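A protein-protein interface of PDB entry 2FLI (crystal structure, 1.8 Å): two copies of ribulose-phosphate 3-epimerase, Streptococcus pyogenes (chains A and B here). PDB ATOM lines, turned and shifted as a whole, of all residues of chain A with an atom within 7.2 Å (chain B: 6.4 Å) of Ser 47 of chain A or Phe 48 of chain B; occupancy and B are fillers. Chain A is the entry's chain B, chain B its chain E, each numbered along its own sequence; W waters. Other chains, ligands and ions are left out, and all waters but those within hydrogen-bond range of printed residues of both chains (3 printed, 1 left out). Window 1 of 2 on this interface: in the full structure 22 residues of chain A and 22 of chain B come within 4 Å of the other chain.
The backbone NH (N) of Gly 49 of chain B sits close to the backbone carbonyl oxygen (O) of Ile 46 of chain A, at 3.4 Å.
The backbone NH (N) of Gly 49 of chain B sits at hydrogen-bond distance from the backbone carbonyl oxygen (O) of Ser 47 of chain A (2.9 Å).
The backbone NH (N) of Gly 49 of chain A sits at hydrogen-bond distance from the backbone carbonyl oxygen (O) of Ser 47 of chain B.
The backbone carbonyl oxygen (O) of Leu 11 of chain B is in hydrogen-bond range of the side-chain hydroxyl (OH) of Tyr 15 of chain B (2.4 Å).
N of Met 38 of chain B is in hydrogen-bond range of OG of Ser 47 of chain B (2.7 Å).
The backbone NH (N) of Met 38 of chain A lies within hydrogen-bond range of the side-chain hydroxyl (OG) of Ser 47 of chain A (2.9 Å).
The side-chain hydroxyl (OG) of Ser 47 of chain A is in hydrogen-bond range of the backbone carbonyl oxygen (O) of Asp 36 of chain A, at 2.7 Å.
The backbone carbonyl oxygen (O) of Leu 11 of chain A is in hydrogen-bond range of the side-chain hydroxyl (OH) of Tyr 15 of chain A (2.5 Å).
The backbone carbonyl oxygen (O) of Asp 36 of chain B lies within hydrogen-bond range of the side-chain hydroxyl (OG) of Ser 47 of chain B (2.7 Å).
Tyr 15 of chain A touches Val 52 of chain B (CD2 to CA, 3.7 Å).
Tyr 15 of chain B touches Phe 18 of chain A (O to CD2, 3.4 Å).
CD1 of Ile 46 of chain B touches CB of Asp 39 of chain A, at 3.5 Å.
Ile 46 of chain A touches Ile 46 of chain B (CG2 to CG2, 3.98 Å).
Ile 46 of chain A touches Phe 48 of chain B.
Phe 48 of chain A touches Ile 46 of chain B.
O of Ser 47 of chain B touches CA of Phe 48 of chain A (3.2 Å).
Gly 49 of chain A touches Ile 46 of chain B (CA to O, 3.3 Å).
Tyr 15 of chain B touches Val 52 of chain A.
Val 70 of chain A touches Ile 46 of chain B (CG1 to CD1, 3.99 Å).
Of chain B, only Phe 48 (3.1 Å), Gly 49 (2.9 Å) and Val 52 (3.7 Å) come within 4 Å of Ser 47 of chain A.
Phe 48 of chain B touches just these residues of chain A: Ile 46 and Ser 47.
Ser 47 of chain B touches just these residues of chain A: Phe 48 (3.2 Å), Gly 49 (2.9 Å) and Val 52 (3.7 Å).
Of the printed residues of chain A, Gly 49 of chain B touches Ile 46 and Ser 47.
Of the printed residues of chain B, Phe 18 of chain A touches Tyr 15 (3.4 Å).
The nearest residue of chain B that does not touch Ser 47 of chain A is Ser 47 of chain B (4.3 Å).
The nearest residue of chain A that does not touch Phe 48 of chain B is Phe 48 of chain A (4.1 Å).
Along chain A the printed residues that touch a printed residue of chain B span positions 15 to 70.
Tyr 15 of chain A touches Phe 18 of chain B, and with the chains exchanged Phe 18 of chain A touches Tyr 15 of chain B.
Ile 46 of chain A touches its own counterpart, Ile 46 of chain B.
Ser 47 of chain A touches Phe 48 of chain B, and with the chains exchanged Phe 48 of chain A touches Ser 47 of chain B.
Ser 47 of chain A touches Gly 49 of chain B, and with the chains exchanged Gly 49 of chain A touches Ser 47 of chain B.
Of the 18 pairs that touch across the chains among the printed residues, 15 have their exchanged pair printed and touching as well.
Water W1 lies within hydrogen-bond range of O of Tyr 15 of chain B (2.7 Å), O of Tyr 15 of chain A (2.8 Å), N of Phe 18 of chain B (3.1 Å) and N of Phe 18 of chain A (3.1 Å).
Water W3 lies within hydrogen-bond range of the backbone carbonyl oxygen of Ile 46 of chain B, the backbone NH of Val 52 of chain A and the backbone carbonyl oxygen of Ser 47 of chain B.
Water W2 bridges O of Ile 46 of chain A (3.1 Å) and N of Asp 51 of chain B (3.2 Å).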
ATOM      1  N   LEU A  11      -8.354 -21.884   7.840  1.00  0.00           N
ATOM      2  CA  LEU A  11      -8.517 -21.279   9.162  1.00  0.00           C
ATOM      3  C   LEU A  11      -7.189 -21.261   9.926  1.00  0.00           C
ATOM      4  O   LEU A  11      -7.010 -20.476  10.848  1.00  0.00           O
ATOM      5  CB  LEU A  11      -9.548 -22.058   9.988  1.00  0.00           C
ATOM      6  CG  LEU A  11      -9.924 -21.432  11.333  1.00  0.00           C
ATOM      7  CD1 LEU A  11     -10.884 -20.270  11.102  1.00  0.00           C
ATOM      8  CD2 LEU A  11     -10.570 -22.473  12.226  1.00  0.00           C
ATOM      9  N   TYR A  15      -4.122 -15.059   7.851  1.00  0.00           N
ATOM     10  CA  TYR A  15      -5.279 -14.303   7.385  1.00  0.00           C
ATOM     11  C   TYR A  15      -4.946 -12.996   6.675  1.00  0.00           C
ATOM     12  O   TYR A  15      -5.762 -12.495   5.903  1.00  0.00           O
ATOM     13  CB  TYR A  15      -6.221 -13.982   8.545  1.00  0.00           C
ATOM     14  CG  TYR A  15      -6.700 -15.181   9.336  1.00  0.00           C
ATOM     15  CD1 TYR A  15      -6.817 -16.437   8.744  1.00  0.00           C
ATOM     16  CD2 TYR A  15      -7.114 -15.038  10.660  1.00  0.00           C
ATOM     17  CE1 TYR A  15      -7.343 -17.515   9.444  1.00  0.00           C
ATOM     18  CE2 TYR A  15      -7.639 -16.115  11.368  1.00  0.00           C
ATOM     19  CZ  TYR A  15      -7.754 -17.349  10.752  1.00  0.00           C
ATOM     20  OH  TYR A  15      -8.290 -18.410  11.442  1.00  0.00           O
ATOM     21  N   PHE A  18      -4.256 -14.126   2.436  1.00  0.00           N
ATOM     22  CA  PHE A  18      -4.988 -15.279   1.933  1.00  0.00           C
ATOM     23  C   PHE A  18      -4.493 -15.699   0.550  1.00  0.00           C
ATOM     24  O   PHE A  18      -4.372 -16.893   0.261  1.00  0.00           O
ATOM     25  CB  PHE A  18      -6.492 -14.980   1.890  1.00  0.00           C
ATOM     26  CG  PHE A  18      -7.179 -15.099   3.236  1.00  0.00           C
ATOM     27  CD1 PHE A  18      -7.086 -16.274   3.983  1.00  0.00           C
ATOM     28  CD2 PHE A  18      -7.946 -14.056   3.737  1.00  0.00           C
ATOM     29  CE1 PHE A  18      -7.749 -16.405   5.208  1.00  0.00           C
ATOM     30  CE2 PHE A  18      -8.613 -14.177   4.959  1.00  0.00           C
ATOM     31  CZ  PHE A  18      -8.514 -15.352   5.693  1.00  0.00           C
ATOM     32  N   ILE A  35     -12.741 -24.353   3.963  1.00  0.00           N
ATOM     33  CA  ILE A  35     -12.990 -23.001   4.460  1.00  0.00           C
ATOM     34  C   ILE A  35     -14.028 -22.978   5.581  1.00  0.00           C
ATOM     35  O   ILE A  35     -15.219 -23.204   5.355  1.00  0.00           O
ATOM     36  CB  ILE A  35     -13.460 -22.093   3.308  1.00  0.00           C
ATOM     37  CG1 ILE A  35     -12.491 -22.223   2.127  1.00  0.00           C
ATOM     38  CG2 ILE A  35     -13.530 -20.645   3.774  1.00  0.00           C
ATOM     39  CD1 ILE A  35     -12.928 -21.479   0.882  1.00  0.00           C
ATOM     40  N   ASP A  36     -13.567 -22.696   6.792  1.00  0.00           N
ATOM     41  CA  ASP A  36     -14.453 -22.667   7.947  1.00  0.00           C
ATOM     42  C   ASP A  36     -15.155 -21.345   8.211  1.00  0.00           C
ATOM     43  O   ASP A  36     -14.522 -20.339   8.539  1.00  0.00           O
ATOM     44  CB  ASP A  36     -13.682 -23.105   9.181  1.00  0.00           C
ATOM     45  CG  ASP A  36     -13.238 -24.537   9.079  1.00  0.00           C
ATOM     46  OD1 ASP A  36     -14.124 -25.387   8.899  1.00  0.00           O
ATOM     47  OD2 ASP A  36     -12.022 -24.810   9.158  1.00  0.00           O
ATOM     48  N   ILE A  37     -16.478 -21.373   8.072  1.00  0.00           N
ATOM     49  CA  ILE A  37     -17.312 -20.200   8.294  1.00  0.00           C
ATOM     50  C   ILE A  37     -17.900 -20.300   9.704  1.00  0.00           C
ATOM     51  O   ILE A  37     -18.589 -21.275  10.019  1.00  0.00           O
ATOM     52  CB  ILE A  37     -18.480 -20.140   7.272  1.00  0.00           C
ATOM     53  CG1 ILE A  37     -17.956 -20.352   5.846  1.00  0.00           C
ATOM     54  CG2 ILE A  37     -19.215 -18.817   7.411  1.00  0.00           C
ATOM     55  CD1 ILE A  37     -16.780 -19.437   5.439  1.00  0.00           C
ATOM     56  N   MET A  38     -17.628 -19.298  10.542  1.00  0.00           N
ATOM     57  CA  MET A  38     -18.119 -19.287  11.925  1.00  0.00           C
ATOM     58  C   MET A  38     -18.795 -17.952  12.225  1.00  0.00           C
ATOM     59  O   MET A  38     -18.203 -16.890  12.007  1.00  0.00           O
ATOM     60  CB  MET A  38     -16.958 -19.503  12.898  1.00  0.00           C
ATOM     61  CG  MET A  38     -16.150 -20.778  12.653  1.00  0.00           C
ATOM     62  SD  MET A  38     -14.870 -21.002  13.913  1.00  0.00           S
ATOM     63  CE  MET A  38     -13.434 -20.474  13.047  1.00  0.00           C
ATOM     64  N   ASP A  39     -20.014 -18.012  12.759  1.00  0.00           N
ATOM     65  CA  ASP A  39     -20.797 -16.811  13.042  1.00  0.00           C
ATOM     66  C   ASP A  39     -20.948 -16.332  14.486  1.00  0.00           C
ATOM     67  O   ASP A  39     -21.780 -15.479  14.750  1.00  0.00           O
ATOM     68  CB  ASP A  39     -22.204 -16.980  12.471  1.00  0.00           C
ATOM     69  CG  ASP A  39     -23.035 -17.999  13.250  1.00  0.00           C
ATOM     70  OD1 ASP A  39     -24.237 -18.113  12.950  1.00  0.00           O
ATOM     71  OD2 ASP A  39     -22.495 -18.681  14.157  1.00  0.00           O
ATOM     72  N   GLY A  40     -20.172 -16.862  15.418  1.00  0.00           N
ATOM     73  CA  GLY A  40     -20.314 -16.409  16.790  1.00  0.00           C
ATOM     74  C   GLY A  40     -21.585 -16.918  17.448  1.00  0.00           C
ATOM     75  O   GLY A  40     -21.818 -16.628  18.620  1.00  0.00           O
ATOM     76  N   VAL A  43     -20.898 -21.465  16.988  1.00  0.00           N
ATOM     77  CA  VAL A  43     -19.691 -21.639  17.775  1.00  0.00           C
ATOM     78  C   VAL A  43     -19.403 -20.248  18.329  1.00  0.00           C
ATOM     79  O   VAL A  43     -19.932 -19.253  17.828  1.00  0.00           O
ATOM     80  CB  VAL A  43     -18.487 -22.155  16.940  1.00  0.00           C
ATOM     81  CG1 VAL A  43     -18.679 -23.641  16.613  1.00  0.00           C
ATOM     82  CG2 VAL A  43     -18.342 -21.338  15.664  1.00  0.00           C
ATOM     83  N   ASN A  45     -16.732 -18.152  18.226  1.00  0.00           N
ATOM     84  CA  ASN A  45     -16.067 -17.157  17.404  1.00  0.00           C
ATOM     85  C   ASN A  45     -16.602 -16.893  16.005  1.00  0.00           C
ATOM     86  O   ASN A  45     -17.413 -17.648  15.466  1.00  0.00           O
ATOM     87  CB  ASN A  45     -14.581 -17.499  17.321  1.00  0.00           C
ATOM     88  CG  ASN A  45     -13.948 -17.627  18.689  1.00  0.00           C
ATOM     89  OD1 ASN A  45     -14.074 -16.734  19.532  1.00  0.00           O
ATOM     90  ND2 ASN A  45     -13.268 -18.739  18.922  1.00  0.00           N
ATOM     91  N   ILE A  46     -16.136 -15.780  15.447  1.00  0.00           N
ATOM     92  CA  ILE A  46     -16.489 -15.350  14.103  1.00  0.00           C
ATOM     93  C   ILE A  46     -15.207 -15.459  13.284  1.00  0.00           C
ATOM     94  O   ILE A  46     -14.194 -14.845  13.634  1.00  0.00           O
ATOM     95  CB  ILE A  46     -16.939 -13.868  14.071  1.00  0.00           C
ATOM     96  CG1 ILE A  46     -18.154 -13.659  14.984  1.00  0.00           C
ATOM     97  CG2 ILE A  46     -17.267 -13.470  12.634  1.00  0.00           C
ATOM     98  CD1 ILE A  46     -18.431 -12.208  15.319  1.00  0.00           C
ATOM     99  N   SER A  47     -15.230 -16.244  12.212  1.00  0.00           N
ATOM    100  CA  SER A  47     -14.048 -16.368  11.376  1.00  0.00           C
ATOM    101  C   SER A  47     -14.185 -15.365  10.234  1.00  0.00           C
ATOM    102  O   SER A  47     -13.737 -14.223  10.351  1.00  0.00           O
ATOM    103  CB  SER A  47     -13.895 -17.800  10.843  1.00  0.00           C
ATOM    104  OG  SER A  47     -15.003 -18.200  10.051  1.00  0.00           O
ATOM    105  N   PHE A  48     -14.824 -15.775   9.144  1.00  0.00           N
ATOM    106  CA  PHE A  48     -15.028 -14.899   7.990  1.00  0.00           C
ATOM    107  C   PHE A  48     -16.245 -15.383   7.203  1.00  0.00           C
ATOM    108  O   PHE A  48     -16.630 -16.546   7.322  1.00  0.00           O
ATOM    109  CB  PHE A  48     -13.770 -14.884   7.104  1.00  0.00           C
ATOM    110  CG  PHE A  48     -12.946 -16.131   7.215  1.00  0.00           C
ATOM    111  CD1 PHE A  48     -13.323 -17.296   6.561  1.00  0.00           C
ATOM    112  CD2 PHE A  48     -11.810 -16.154   8.020  1.00  0.00           C
ATOM    113  CE1 PHE A  48     -12.584 -18.471   6.709  1.00  0.00           C
ATOM    114  CE2 PHE A  48     -11.063 -17.325   8.175  1.00  0.00           C
ATOM    115  CZ  PHE A  48     -11.450 -18.484   7.519  1.00  0.00           C
ATOM    116  N   GLY A  49     -16.837 -14.491   6.410  1.00  0.00           N
ATOM    117  CA  GLY A  49     -18.026 -14.835   5.648  1.00  0.00           C
ATOM    118  C   GLY A  49     -17.917 -15.031   4.142  1.00  0.00           C
ATOM    119  O   GLY A  49     -16.830 -15.232   3.594  1.00  0.00           O
ATOM    120  N   VAL A  52     -15.572 -12.873   1.981  1.00  0.00           N
ATOM    121  CA  VAL A  52     -14.161 -13.191   2.084  1.00  0.00           C
ATOM    122  C   VAL A  52     -13.915 -14.379   1.156  1.00  0.00           C
ATOM    123  O   VAL A  52     -12.897 -14.435   0.466  1.00  0.00           O
ATOM    124  CB  VAL A  52     -13.761 -13.541   3.534  1.00  0.00           C
ATOM    125  CG1 VAL A  52     -12.388 -14.195   3.563  1.00  0.00           C
ATOM    126  CG2 VAL A  52     -13.739 -12.271   4.374  1.00  0.00           C
ATOM    127  N   HIS A  67     -17.374 -25.079   4.885  1.00  0.00           N
ATOM    128  CA  HIS A  67     -17.996 -25.697   6.049  1.00  0.00           C
ATOM    129  C   HIS A  67     -18.670 -24.595   6.868  1.00  0.00           C
ATOM    130  O   HIS A  67     -17.996 -23.730   7.438  1.00  0.00           O
ATOM    131  CB  HIS A  67     -16.910 -26.394   6.875  1.00  0.00           C
ATOM    132  CG  HIS A  67     -17.407 -27.021   8.140  1.00  0.00           C
ATOM    133  ND1 HIS A  67     -16.553 -27.521   9.099  1.00  0.00           N
ATOM    134  CD2 HIS A  67     -18.660 -27.230   8.608  1.00  0.00           C
ATOM    135  CE1 HIS A  67     -17.258 -28.010  10.104  1.00  0.00           C
ATOM    136  NE2 HIS A  67     -18.539 -27.845   9.831  1.00  0.00           N
ATOM    137  N   MET A  69     -20.311 -23.319  10.019  1.00  0.00           N
ATOM    138  CA  MET A  69     -20.569 -23.472  11.440  1.00  0.00           C
ATOM    139  C   MET A  69     -21.349 -22.227  11.830  1.00  0.00           C
ATOM    140  O   MET A  69     -20.871 -21.375  12.577  1.00  0.00           O
ATOM    141  CB  MET A  69     -19.251 -23.572  12.215  1.00  0.00           C
ATOM    142  CG  MET A  69     -18.576 -24.923  12.005  1.00  0.00           C
ATOM    143  SD  MET A  69     -16.923 -25.022  12.661  1.00  0.00           S
ATOM    144  CE  MET A  69     -15.993 -24.487  11.239  1.00  0.00           C
ATOM    145  N   VAL A  70     -22.551 -22.120  11.277  1.00  0.00           N
ATOM    146  CA  VAL A  70     -23.416 -20.988  11.536  1.00  0.00           C
ATOM    147  C   VAL A  70     -24.845 -21.473  11.729  1.00  0.00           C
ATOM    148  O   VAL A  70     -25.204 -22.564  11.277  1.00  0.00           O
ATOM    149  CB  VAL A  70     -23.375 -19.978  10.354  1.00  0.00           C
ATOM    150  CG1 VAL A  70     -21.935 -19.763   9.910  1.00  0.00           C
ATOM    151  CG2 VAL A  70     -24.238 -20.473   9.190  1.00  0.00           C
ATOM    152  N   ILE B  10     -11.760  -1.012   5.981  1.00  0.00           N
ATOM    153  CA  ILE B  10     -11.150  -2.178   5.373  1.00  0.00           C
ATOM    154  C   ILE B  10     -12.201  -3.108   4.752  1.00  0.00           C
ATOM    155  O   ILE B  10     -11.872  -3.977   3.940  1.00  0.00           O
ATOM    156  CB  ILE B  10     -10.283  -2.930   6.417  1.00  0.00           C
ATOM    157  CG1 ILE B  10      -9.225  -3.768   5.704  1.00  0.00           C
ATOM    158  CG2 ILE B  10     -11.162  -3.798   7.322  1.00  0.00           C
ATOM    159  CD1 ILE B  10      -8.130  -2.935   5.062  1.00  0.00           C
ATOM    160  N   LEU B  11     -13.465  -2.916   5.130  1.00  0.00           N
ATOM    161  CA  LEU B  11     -14.560  -3.722   4.586  1.00  0.00           C
ATOM    162  C   LEU B  11     -14.594  -3.567   3.064  1.00  0.00           C
ATOM    163  O   LEU B  11     -15.087  -4.445   2.352  1.00  0.00           O
ATOM    164  CB  LEU B  11     -15.914  -3.260   5.150  1.00  0.00           C
ATOM    165  CG  LEU B  11     -17.143  -4.050   4.671  1.00  0.00           C
ATOM    166  CD1 LEU B  11     -17.216  -5.377   5.422  1.00  0.00           C
ATOM    167  CD2 LEU B  11     -18.417  -3.248   4.908  1.00  0.00           C
ATOM    168  N   TYR B  15      -9.843  -8.366   0.505  1.00  0.00           N
ATOM    169  CA  TYR B  15      -9.716  -9.335   1.591  1.00  0.00           C
ATOM    170  C   TYR B  15      -8.618 -10.378   1.433  1.00  0.00           C
ATOM    171  O   TYR B  15      -8.132 -10.910   2.431  1.00  0.00           O
ATOM    172  CB  TYR B  15     -11.040 -10.067   1.813  1.00  0.00           C
ATOM    173  CG  TYR B  15     -12.228  -9.174   2.065  1.00  0.00           C
ATOM    174  CD1 TYR B  15     -12.072  -7.898   2.603  1.00  0.00           C
ATOM    175  CD2 TYR B  15     -13.518  -9.624   1.802  1.00  0.00           C
ATOM    176  CE1 TYR B  15     -13.176  -7.094   2.872  1.00  0.00           C
ATOM    177  CE2 TYR B  15     -14.623  -8.832   2.070  1.00  0.00           C
ATOM    178  CZ  TYR B  15     -14.447  -7.570   2.604  1.00  0.00           C
ATOM    179  OH  TYR B  15     -15.553  -6.793   2.863  1.00  0.00           O
ATOM    180  N   PHE B  18      -4.937  -8.486   2.913  1.00  0.00           N
ATOM    181  CA  PHE B  18      -5.091  -7.481   3.959  1.00  0.00           C
ATOM    182  C   PHE B  18      -3.801  -6.726   4.242  1.00  0.00           C
ATOM    183  O   PHE B  18      -3.815  -5.504   4.384  1.00  0.00           O
ATOM    184  CB  PHE B  18      -5.605  -8.118   5.253  1.00  0.00           C
ATOM    185  CG  PHE B  18      -7.090  -8.332   5.274  1.00  0.00           C
ATOM    186  CD1 PHE B  18      -7.955  -7.276   5.010  1.00  0.00           C
ATOM    187  CD2 PHE B  18      -7.626  -9.579   5.575  1.00  0.00           C
ATOM    188  CE1 PHE B  18      -9.332  -7.454   5.044  1.00  0.00           C
ATOM    189  CE2 PHE B  18      -9.002  -9.769   5.613  1.00  0.00           C
ATOM    190  CZ  PHE B  18      -9.856  -8.706   5.347  1.00  0.00           C
ATOM    191  N   ILE B  35     -12.597  -0.990  11.096  1.00  0.00           N
ATOM    192  CA  ILE B  35     -12.807  -2.423  10.908  1.00  0.00           C
ATOM    193  C   ILE B  35     -14.216  -2.881  11.307  1.00  0.00           C
ATOM    194  O   ILE B  35     -14.589  -2.864  12.483  1.00  0.00           O
ATOM    195  CB  ILE B  35     -11.737  -3.219  11.699  1.00  0.00           C
ATOM    196  CG1 ILE B  35     -10.340  -2.693  11.335  1.00  0.00           C
ATOM    197  CG2 ILE B  35     -11.820  -4.698  11.346  1.00  0.00           C
ATOM    198  CD1 ILE B  35      -9.190  -3.348  12.098  1.00  0.00           C
ATOM    199  N   ASP B  36     -14.986  -3.297  10.307  1.00  0.00           N
ATOM    200  CA  ASP B  36     -16.366  -3.742  10.503  1.00  0.00           C
ATOM    201  C   ASP B  36     -16.522  -5.223  10.771  1.00  0.00           C
ATOM    202  O   ASP B  36     -16.259  -6.045   9.897  1.00  0.00           O
ATOM    203  CB  ASP B  36     -17.202  -3.379   9.278  1.00  0.00           C
ATOM    204  CG  ASP B  36     -17.399  -1.897   9.143  1.00  0.00           C
ATOM    205  OD1 ASP B  36     -17.922  -1.308  10.097  1.00  0.00           O
ATOM    206  OD2 ASP B  36     -17.037  -1.326   8.096  1.00  0.00           O
ATOM    207  N   ILE B  37     -16.972  -5.544  11.982  1.00  0.00           N
ATOM    208  CA  ILE B  37     -17.188  -6.923  12.408  1.00  0.00           C
ATOM    209  C   ILE B  37     -18.684  -7.212  12.275  1.00  0.00           C
ATOM    210  O   ILE B  37     -19.506  -6.566  12.924  1.00  0.00           O
ATOM    211  CB  ILE B  37     -16.758  -7.112  13.887  1.00  0.00           C
ATOM    212  CG1 ILE B  37     -15.342  -6.555  14.101  1.00  0.00           C
ATOM    213  CG2 ILE B  37     -16.822  -8.576  14.273  1.00  0.00           C
ATOM    214  CD1 ILE B  37     -14.258  -7.255  13.297  1.00  0.00           C
ATOM    215  N   MET B  38     -19.033  -8.193  11.446  1.00  0.00           N
ATOM    216  CA  MET B  38     -20.434  -8.544  11.223  1.00  0.00           C
ATOM    217  C   MET B  38     -20.662 -10.021  11.515  1.00  0.00           C
ATOM    218  O   MET B  38     -19.942 -10.877  11.005  1.00  0.00           O
ATOM    219  CB  MET B  38     -20.820  -8.231   9.779  1.00  0.00           C
ATOM    220  CG  MET B  38     -20.734  -6.750   9.422  1.00  0.00           C
ATOM    221  SD  MET B  38     -21.113  -6.474   7.669  1.00  0.00           S
ATOM    222  CE  MET B  38     -20.422  -4.840   7.456  1.00  0.00           C
ATOM    223  N   ILE B  46     -21.794 -11.912   7.358  1.00  0.00           N
ATOM    224  CA  ILE B  46     -20.663 -12.188   8.225  1.00  0.00           C
ATOM    225  C   ILE B  46     -19.454 -11.590   7.505  1.00  0.00           C
ATOM    226  O   ILE B  46     -19.251 -11.850   6.320  1.00  0.00           O
ATOM    227  CB  ILE B  46     -20.438 -13.704   8.390  1.00  0.00           C
ATOM    228  CG1 ILE B  46     -21.619 -14.332   9.135  1.00  0.00           C
ATOM    229  CG2 ILE B  46     -19.134 -13.955   9.148  1.00  0.00           C
ATOM    230  CD1 ILE B  46     -21.581 -15.858   9.174  1.00  0.00           C
ATOM    231  N   SER B  47     -18.681 -10.757   8.195  1.00  0.00           N
ATOM    232  CA  SER B  47     -17.497 -10.173   7.570  1.00  0.00           C
ATOM    233  C   SER B  47     -16.274 -10.962   8.036  1.00  0.00           C
ATOM    234  O   SER B  47     -15.831 -11.892   7.360  1.00  0.00           O
ATOM    235  CB  SER B  47     -17.368  -8.682   7.926  1.00  0.00           C
ATOM    236  OG  SER B  47     -17.432  -8.437   9.324  1.00  0.00           O
ATOM    237  N   PHE B  48     -15.746 -10.601   9.195  1.00  0.00           N
ATOM    238  CA  PHE B  48     -14.592 -11.277   9.773  1.00  0.00           C
ATOM    239  C   PHE B  48     -14.565 -10.972  11.266  1.00  0.00           C
ATOM    240  O   PHE B  48     -15.136  -9.967  11.705  1.00  0.00           O
ATOM    241  CB  PHE B  48     -13.296 -10.818   9.084  1.00  0.00           C
ATOM    242  CG  PHE B  48     -13.348  -9.408   8.561  1.00  0.00           C
ATOM    243  CD1 PHE B  48     -13.202  -8.324   9.417  1.00  0.00           C
ATOM    244  CD2 PHE B  48     -13.555  -9.166   7.208  1.00  0.00           C
ATOM    245  CE1 PHE B  48     -13.263  -7.018   8.931  1.00  0.00           C
ATOM    246  CE2 PHE B  48     -13.617  -7.868   6.716  1.00  0.00           C
ATOM    247  CZ  PHE B  48     -13.471  -6.793   7.580  1.00  0.00           C
ATOM    248  N   GLY B  49     -13.914 -11.838  12.040  1.00  0.00           N
ATOM    249  CA  GLY B  49     -13.869 -11.661  13.479  1.00  0.00           C
ATOM    250  C   GLY B  49     -12.546 -11.234  14.103  1.00  0.00           C
ATOM    251  O   GLY B  49     -11.634 -10.750  13.426  1.00  0.00           O
ATOM    252  N   ALA B  50     -12.444 -11.442  15.412  1.00  0.00           N
ATOM    253  CA  ALA B  50     -11.265 -11.053  16.181  1.00  0.00           C
ATOM    254  C   ALA B  50      -9.940 -11.657  15.730  1.00  0.00           C
ATOM    255  O   ALA B  50      -8.916 -10.976  15.749  1.00  0.00           O
ATOM    256  CB  ALA B  50     -11.491 -11.353  17.666  1.00  0.00           C
ATOM    257  N   ASP B  51      -9.938 -12.927  15.333  1.00  0.00           N
ATOM    258  CA  ASP B  51      -8.686 -13.535  14.907  1.00  0.00           C
ATOM    259  C   ASP B  51      -8.178 -12.907  13.626  1.00  0.00           C
ATOM    260  O   ASP B  51      -6.973 -12.860  13.398  1.00  0.00           O
ATOM    261  CB  ASP B  51      -8.840 -15.046  14.749  1.00  0.00           C
ATOM    262  CG  ASP B  51      -8.775 -15.770  16.079  1.00  0.00           C
ATOM    263  OD1 ASP B  51      -9.309 -16.894  16.170  1.00  0.00           O
ATOM    264  OD2 ASP B  51      -8.179 -15.218  17.032  1.00  0.00           O
ATOM    265  N   VAL B  52      -9.091 -12.424  12.787  1.00  0.00           N
ATOM    266  CA  VAL B  52      -8.686 -11.754  11.556  1.00  0.00           C
ATOM    267  C   VAL B  52      -8.075 -10.408  11.950  1.00  0.00           C
ATOM    268  O   VAL B  52      -7.066  -9.989  11.389  1.00  0.00           O
ATOM    269  CB  VAL B  52      -9.888 -11.517  10.609  1.00  0.00           C
ATOM    270  CG1 VAL B  52      -9.507 -10.506   9.524  1.00  0.00           C
ATOM    271  CG2 VAL B  52     -10.319 -12.841   9.973  1.00  0.00           C
ATOM    272  N   VAL B  53      -8.686  -9.736  12.923  1.00  0.00           N
ATOM    273  CA  VAL B  53      -8.170  -8.445  13.374  1.00  0.00           C
ATOM    274  C   VAL B  53      -6.780  -8.619  13.991  1.00  0.00           C
ATOM    275  O   VAL B  53      -5.882  -7.803  13.763  1.00  0.00           O
ATOM    276  CB  VAL B  53      -9.102  -7.781  14.426  1.00  0.00           C
ATOM    277  CG1 VAL B  53      -8.478  -6.486  14.930  1.00  0.00           C
ATOM    278  CG2 VAL B  53     -10.460  -7.492  13.818  1.00  0.00           C
ATOM    279  N   MET B  56      -4.308  -8.727  11.321  1.00  0.00           N
ATOM    280  CA  MET B  56      -4.093  -7.417  10.704  1.00  0.00           C
ATOM    281  C   MET B  56      -3.200  -6.536  11.577  1.00  0.00           C
ATOM    282  O   MET B  56      -2.404  -5.742  11.075  1.00  0.00           O
ATOM    283  CB  MET B  56      -5.426  -6.678  10.515  1.00  0.00           C
ATOM    284  CG  MET B  56      -6.424  -7.329   9.571  1.00  0.00           C
ATOM    285  SD  MET B  56      -7.962  -6.369   9.487  1.00  0.00           S
ATOM    286  CE  MET B  56      -9.039  -7.321  10.505  1.00  0.00           C
ATOM    287  N   PHE B  80     -10.985  -8.796  21.457  1.00  0.00           N
ATOM    288  CA  PHE B  80     -10.527  -7.635  20.707  1.00  0.00           C
ATOM    289  C   PHE B  80      -9.365  -6.930  21.384  1.00  0.00           C
ATOM    290  O   PHE B  80      -8.508  -6.343  20.718  1.00  0.00           O
ATOM    291  CB  PHE B  80     -11.697  -6.682  20.447  1.00  0.00           C
ATOM    292  CG  PHE B  80     -12.470  -7.040  19.222  1.00  0.00           C
ATOM    293  CD1 PHE B  80     -12.096  -6.540  17.982  1.00  0.00           C
ATOM    294  CD2 PHE B  80     -13.501  -7.969  19.286  1.00  0.00           C
ATOM    295  CE1 PHE B  80     -12.731  -6.963  16.825  1.00  0.00           C
ATOM    296  CE2 PHE B  80     -14.139  -8.399  18.138  1.00  0.00           C
ATOM    297  CZ  PHE B  80     -13.755  -7.897  16.903  1.00  0.00           C
HETATM  298  O   HOH W   1      -5.661 -11.461   3.312  1.00  0.00           O
HETATM  299  O   HOH W   2     -12.196 -15.163  15.938  1.00  0.00           O
HETATM  300  O   HOH W   3     -17.190 -11.675   4.354  1.00  0.00           O
